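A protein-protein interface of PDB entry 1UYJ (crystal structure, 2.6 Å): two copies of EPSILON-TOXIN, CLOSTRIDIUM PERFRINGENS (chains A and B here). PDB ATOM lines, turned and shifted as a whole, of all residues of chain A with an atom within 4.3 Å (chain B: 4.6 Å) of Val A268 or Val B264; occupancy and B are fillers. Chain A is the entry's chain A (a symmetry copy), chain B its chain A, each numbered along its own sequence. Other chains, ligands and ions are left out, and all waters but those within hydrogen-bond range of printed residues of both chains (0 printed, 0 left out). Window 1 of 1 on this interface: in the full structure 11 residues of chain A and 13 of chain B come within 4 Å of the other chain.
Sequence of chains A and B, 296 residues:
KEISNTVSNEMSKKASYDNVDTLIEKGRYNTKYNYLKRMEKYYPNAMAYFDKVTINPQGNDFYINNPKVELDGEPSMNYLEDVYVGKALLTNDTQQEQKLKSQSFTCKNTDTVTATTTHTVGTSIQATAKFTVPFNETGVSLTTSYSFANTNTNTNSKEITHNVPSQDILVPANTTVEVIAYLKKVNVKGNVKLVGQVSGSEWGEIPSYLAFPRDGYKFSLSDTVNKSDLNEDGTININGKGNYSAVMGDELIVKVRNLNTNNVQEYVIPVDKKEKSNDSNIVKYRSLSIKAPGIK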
ATOM      1  N   GLU A 251      19.311  -6.377 -19.657  1.00  0.00           N
ATOM      2  CA  GLU A 251      19.284  -6.049 -21.053  1.00  0.00           C
ATOM      3  C   GLU A 251      20.396  -5.064 -21.421  1.00  0.00           C
ATOM      4  O   GLU A 251      20.866  -4.289 -20.575  1.00  0.00           O
ATOM      5  CB  GLU A 251      17.881  -5.563 -21.449  1.00  0.00           C
ATOM      6  CG  GLU A 251      16.780  -6.631 -21.278  1.00  0.00           C
ATOM      7  CD  GLU A 251      15.360  -6.142 -21.561  1.00  0.00           C
ATOM      8  OE1 GLU A 251      15.057  -4.924 -21.619  1.00  0.00           O
ATOM      9  OE2 GLU A 251      14.495  -6.991 -21.739  1.00  0.00           O
ATOM     10  N   LEU A 252      20.858  -5.177 -22.668  1.00  0.00           N
ATOM     11  CA  LEU A 252      21.739  -4.194 -23.299  1.00  0.00           C
ATOM     12  C   LEU A 252      20.855  -3.166 -23.959  1.00  0.00           C
ATOM     13  O   LEU A 252      19.987  -3.530 -24.760  1.00  0.00           O
ATOM     14  CB  LEU A 252      22.633  -4.819 -24.374  1.00  0.00           C
ATOM     15  CG  LEU A 252      23.811  -3.889 -24.746  1.00  0.00           C
ATOM     16  CD1 LEU A 252      25.147  -4.360 -24.128  1.00  0.00           C
ATOM     17  CD2 LEU A 252      23.956  -3.751 -26.253  1.00  0.00           C
ATOM     18  N   GLU A 266      14.649   4.616 -27.201  1.00  0.00           N
ATOM     19  CA  GLU A 266      15.383   3.602 -26.451  1.00  0.00           C
ATOM     20  C   GLU A 266      15.128   2.253 -27.115  1.00  0.00           C
ATOM     21  O   GLU A 266      14.025   1.994 -27.620  1.00  0.00           O
ATOM     22  CB  GLU A 266      14.906   3.629 -24.993  1.00  0.00           C
ATOM     23  CG  GLU A 266      15.251   2.418 -24.133  1.00  0.00           C
ATOM     24  CD  GLU A 266      14.681   2.520 -22.723  1.00  0.00           C
ATOM     25  OE1 GLU A 266      13.950   3.493 -22.447  1.00  0.00           O
ATOM     26  OE2 GLU A 266      14.955   1.626 -21.878  1.00  0.00           O
ATOM     27  N   TYR A 267      16.157   1.406 -27.114  1.00  0.00           N
ATOM     28  CA  TYR A 267      16.141   0.121 -27.799  1.00  0.00           C
ATOM     29  C   TYR A 267      16.887  -0.933 -27.017  1.00  0.00           C
ATOM     30  O   TYR A 267      17.933  -0.660 -26.430  1.00  0.00           O
ATOM     31  CB  TYR A 267      16.830   0.250 -29.149  1.00  0.00           C
ATOM     32  CG  TYR A 267      16.045   1.034 -30.154  1.00  0.00           C
ATOM     33  CD1 TYR A 267      15.105   0.403 -30.945  1.00  0.00           C
ATOM     34  CD2 TYR A 267      16.232   2.394 -30.317  1.00  0.00           C
ATOM     35  CE1 TYR A 267      14.367   1.097 -31.870  1.00  0.00           C
ATOM     36  CE2 TYR A 267      15.492   3.100 -31.249  1.00  0.00           C
ATOM     37  CZ  TYR A 267      14.555   2.425 -32.012  1.00  0.00           C
ATOM     38  OH  TYR A 267      13.812   3.041 -32.964  1.00  0.00           O
ATOM     39  N   VAL A 268      16.359  -2.148 -27.021  1.00  0.00           N
ATOM     40  CA  VAL A 268      17.057  -3.264 -26.449  1.00  0.00           C
ATOM     41  C   VAL A 268      17.678  -3.980 -27.636  1.00  0.00           C
ATOM     42  O   VAL A 268      17.002  -4.208 -28.634  1.00  0.00           O
ATOM     43  CB  VAL A 268      16.099  -4.183 -25.696  1.00  0.00           C
ATOM     44  CG1 VAL A 268      16.782  -5.493 -25.297  1.00  0.00           C
ATOM     45  CG2 VAL A 268      15.504  -3.470 -24.462  1.00  0.00           C
ATOM     46  N   ILE A 269      18.980  -4.256 -27.535  1.00  0.00           N
ATOM     47  CA  ILE A 269      19.694  -5.094 -28.483  1.00  0.00           C
ATOM     48  C   ILE A 269      19.697  -6.535 -27.918  1.00  0.00           C
ATOM     49  O   ILE A 269      20.402  -6.811 -26.929  1.00  0.00           O
ATOM     50  CB  ILE A 269      21.150  -4.576 -28.709  1.00  0.00           C
ATOM     51  CG1 ILE A 269      21.235  -3.451 -29.756  1.00  0.00           C
ATOM     52  CG2 ILE A 269      22.028  -5.685 -29.286  1.00  0.00           C
ATOM     53  CD1 ILE A 269      20.306  -2.331 -29.608  1.00  0.00           C
ATOM     54  N   PRO A 270      18.909  -7.444 -28.511  1.00  0.00           N
ATOM     55  CA  PRO A 270      18.798  -8.809 -27.980  1.00  0.00           C
ATOM     56  C   PRO A 270      20.053  -9.645 -28.148  1.00  0.00           C
ATOM     57  O   PRO A 270      20.857  -9.408 -29.047  1.00  0.00           O
ATOM     58  CB  PRO A 270      17.642  -9.436 -28.784  1.00  0.00           C
ATOM     59  CG  PRO A 270      17.022  -8.327 -29.553  1.00  0.00           C
ATOM     60  CD  PRO A 270      18.062  -7.254 -29.704  1.00  0.00           C
ATOM     61  N   LEU A 288      20.964  -5.140 -35.316  1.00  0.00           N
ATOM     62  CA  LEU A 288      19.616  -4.656 -35.535  1.00  0.00           C
ATOM     63  C   LEU A 288      19.672  -3.513 -36.502  1.00  0.00           C
ATOM     64  O   LEU A 288      20.706  -2.876 -36.654  1.00  0.00           O
ATOM     65  CB  LEU A 288      19.039  -4.150 -34.228  1.00  0.00           C
ATOM     66  CG  LEU A 288      18.078  -5.049 -33.471  1.00  0.00           C
ATOM     67  CD1 LEU A 288      18.446  -6.520 -33.582  1.00  0.00           C
ATOM     68  CD2 LEU A 288      18.042  -4.582 -32.018  1.00  0.00           C
ATOM     69  N   LYS B 255       7.106  -0.435 -18.891  1.00  0.00           N
ATOM     70  CA  LYS B 255       7.875  -0.315 -20.131  1.00  0.00           C
ATOM     71  C   LYS B 255       7.459  -1.462 -21.036  1.00  0.00           C
ATOM     72  O   LYS B 255       7.520  -2.609 -20.629  1.00  0.00           O
ATOM     73  CB  LYS B 255       9.372  -0.403 -19.824  1.00  0.00           C
ATOM     74  CG  LYS B 255      10.063   0.932 -19.804  1.00  0.00           C
ATOM     75  CD  LYS B 255      11.532   0.813 -19.381  1.00  0.00           C
ATOM     76  N   VAL B 256       7.025  -1.160 -22.250  1.00  0.00           N
ATOM     77  CA  VAL B 256       6.687  -2.206 -23.209  1.00  0.00           C
ATOM     78  C   VAL B 256       7.561  -2.089 -24.436  1.00  0.00           C
ATOM     79  O   VAL B 256       7.729  -1.021 -25.015  1.00  0.00           O
ATOM     80  CB  VAL B 256       5.153  -2.232 -23.586  1.00  0.00           C
ATOM     81  CG1 VAL B 256       4.585  -0.879 -23.655  1.00  0.00           C
ATOM     82  CG2 VAL B 256       4.898  -2.971 -24.921  1.00  0.00           C
ATOM     83  N   ARG B 257       8.061  -3.234 -24.851  1.00  0.00           N
ATOM     84  CA  ARG B 257       9.007  -3.369 -25.926  1.00  0.00           C
ATOM     85  C   ARG B 257       8.429  -4.269 -27.012  1.00  0.00           C
ATOM     86  O   ARG B 257       7.993  -5.382 -26.751  1.00  0.00           O
ATOM     87  CB  ARG B 257      10.238  -4.010 -25.345  1.00  0.00           C
ATOM     88  CG  ARG B 257      11.324  -4.390 -26.313  1.00  0.00           C
ATOM     89  CD  ARG B 257      12.614  -4.724 -25.585  1.00  0.00           C
ATOM     90  NE  ARG B 257      13.390  -5.665 -26.347  1.00  0.00           N
ATOM     91  CZ  ARG B 257      13.775  -6.864 -25.934  1.00  0.00           C
ATOM     92  NH1 ARG B 257      13.490  -7.347 -24.718  1.00  0.00           N
ATOM     93  NH2 ARG B 257      14.473  -7.602 -26.787  1.00  0.00           N
ATOM     94  N   ASN B 262      12.210  -3.791 -31.579  1.00  0.00           N
ATOM     95  CA  ASN B 262      12.923  -3.569 -30.315  1.00  0.00           C
ATOM     96  C   ASN B 262      12.817  -2.168 -29.736  1.00  0.00           C
ATOM     97  O   ASN B 262      13.524  -1.864 -28.793  1.00  0.00           O
ATOM     98  CB  ASN B 262      14.401  -3.974 -30.422  1.00  0.00           C
ATOM     99  CG  ASN B 262      14.586  -5.458 -30.600  1.00  0.00           C
ATOM    100  OD1 ASN B 262      14.916  -5.928 -31.687  1.00  0.00           O
ATOM    101  ND2 ASN B 262      14.398  -6.204 -29.527  1.00  0.00           N
ATOM    102  N   ASN B 263      11.943  -1.317 -30.264  1.00  0.00           N
ATOM    103  CA  ASN B 263      11.708  -0.016 -29.642  1.00  0.00           C
ATOM    104  C   ASN B 263      11.005  -0.198 -28.291  1.00  0.00           C
ATOM    105  O   ASN B 263      10.160  -1.078 -28.149  1.00  0.00           O
ATOM    106  CB  ASN B 263      10.897   0.892 -30.569  1.00  0.00           C
ATOM    107  CG  ASN B 263      10.783   2.312 -30.042  1.00  0.00           C
ATOM    108  OD1 ASN B 263      11.767   2.903 -29.605  1.00  0.00           O
ATOM    109  ND2 ASN B 263       9.580   2.851 -30.046  1.00  0.00           N
ATOM    110  N   VAL B 264      11.358   0.618 -27.299  1.00  0.00           N
ATOM    111  CA  VAL B 264      10.710   0.562 -25.975  1.00  0.00           C
ATOM    112  C   VAL B 264       9.983   1.856 -25.702  1.00  0.00           C
ATOM    113  O   VAL B 264      10.558   2.917 -25.866  1.00  0.00           O
ATOM    114  CB  VAL B 264      11.728   0.340 -24.865  1.00  0.00           C
ATOM    115  CG1 VAL B 264      11.035  -0.032 -23.566  1.00  0.00           C
ATOM    116  CG2 VAL B 264      12.735  -0.754 -25.268  1.00  0.00           C
ATOM    117  N   GLN B 265       8.707   1.776 -25.339  1.00  0.00           N
ATOM    118  CA  GLN B 265       7.930   2.954 -24.922  1.00  0.00           C
ATOM    119  C   GLN B 265       7.636   2.831 -23.436  1.00  0.00           C
ATOM    120  O   GLN B 265       7.480   1.750 -22.930  1.00  0.00           O
ATOM    121  CB  GLN B 265       6.614   3.066 -25.710  1.00  0.00           C
ATOM    122  CG  GLN B 265       6.730   3.624 -27.139  1.00  0.00           C
ATOM    123  CD  GLN B 265       7.335   5.014 -27.188  1.00  0.00           C
ATOM    124  OE1 GLN B 265       8.493   5.171 -27.579  1.00  0.00           O
ATOM    125  NE2 GLN B 265       6.558   6.025 -26.793  1.00  0.00           N
ATOM    126  N   GLU B 266       7.548   3.948 -22.745  1.00  0.00           N
ATOM    127  CA  GLU B 266       7.512   3.981 -21.286  1.00  0.00           C
ATOM    128  C   GLU B 266       6.206   4.645 -20.866  1.00  0.00           C
ATOM    129  O   GLU B 266       5.724   5.573 -21.533  1.00  0.00           O
ATOM    130  CB  GLU B 266       8.741   4.749 -20.783  1.00  0.00           C
ATOM    131  CG  GLU B 266       8.706   5.231 -19.336  1.00  0.00           C
ATOM    132  CD  GLU B 266       9.946   6.032 -18.956  1.00  0.00           C
ATOM    133  OE1 GLU B 266      10.789   6.278 -19.843  1.00  0.00           O
ATOM    134  OE2 GLU B 266      10.090   6.425 -17.768  1.00  0.00           O
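The backbone carbonyl oxygen of Asn B262 is in hydrogen-bond range of the backbone NH of Val A268, at 3.4 Å.
The backbone NH (N) of Val B264 sits at hydrogen-bond distance from the backbone carbonyl oxygen (O) of Glu A266 (3.0 Å).
The guanidinium group of Arg B257 is in salt-bridge range of the side-chain carboxylate of Glu A251.
The backbone carbonyl oxygen (O) of Glu A266 sits close to the side-chain amide oxygen (OD1) of Asn B263.
The guanidinium group (NH2) of Arg B257 sits close to the side-chain amide nitrogen (ND2) of Asn B262 (3.1 Å).
Tyr A267 touches Asn B262 (CA to O, 3.4 Å).
Asn B263 touches Tyr A267 (CA to CE1, 3.6 Å).
Val A268 touches Arg B257 (CB to NE, 3.2 Å).
CG2 of Val A268 touches CG2 of Val B264, 3.96 Å away.
Arg B257 touches Pro A270 (NH2 to CG, 3.8 Å).
ND2 of Asn B262 touches CG of Pro A270, at 3.4 Å.
OD1 of Asn B262 touches CD2 of Leu A288, 3.4 Å away.
Printed residues of chain B within 4 Å of Glu A266: Asn B263 (3.1 Å) and Val B264 (3.0 Å).
Of the printed residues of chain B, Val A268 touches Arg B257 (3.2 Å), Asn B262 (3.2 Å) and Val B264 (3.96 Å).
Ile A269 touches none of the printed residues of chain B.
Printed residues of chain B within 4 Å of Leu A288: Asn B262 (3.4 Å).
Lys B255 touches none of the printed residues of chain A.
Printed residues of chain A within 4 Å of Asn B263: Glu A266 and Tyr A267.
Val B264 touches just these residues of chain A: Glu A266 and Val A268.
Hydrophobic or aromatic side chains of chain B that line the printed part of chain A: Val B264.
Position printed for both chains: 266.
Of the 11 pairs that touch across the chains among the printed residues, none has its exchanged pair printed and touching as well.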
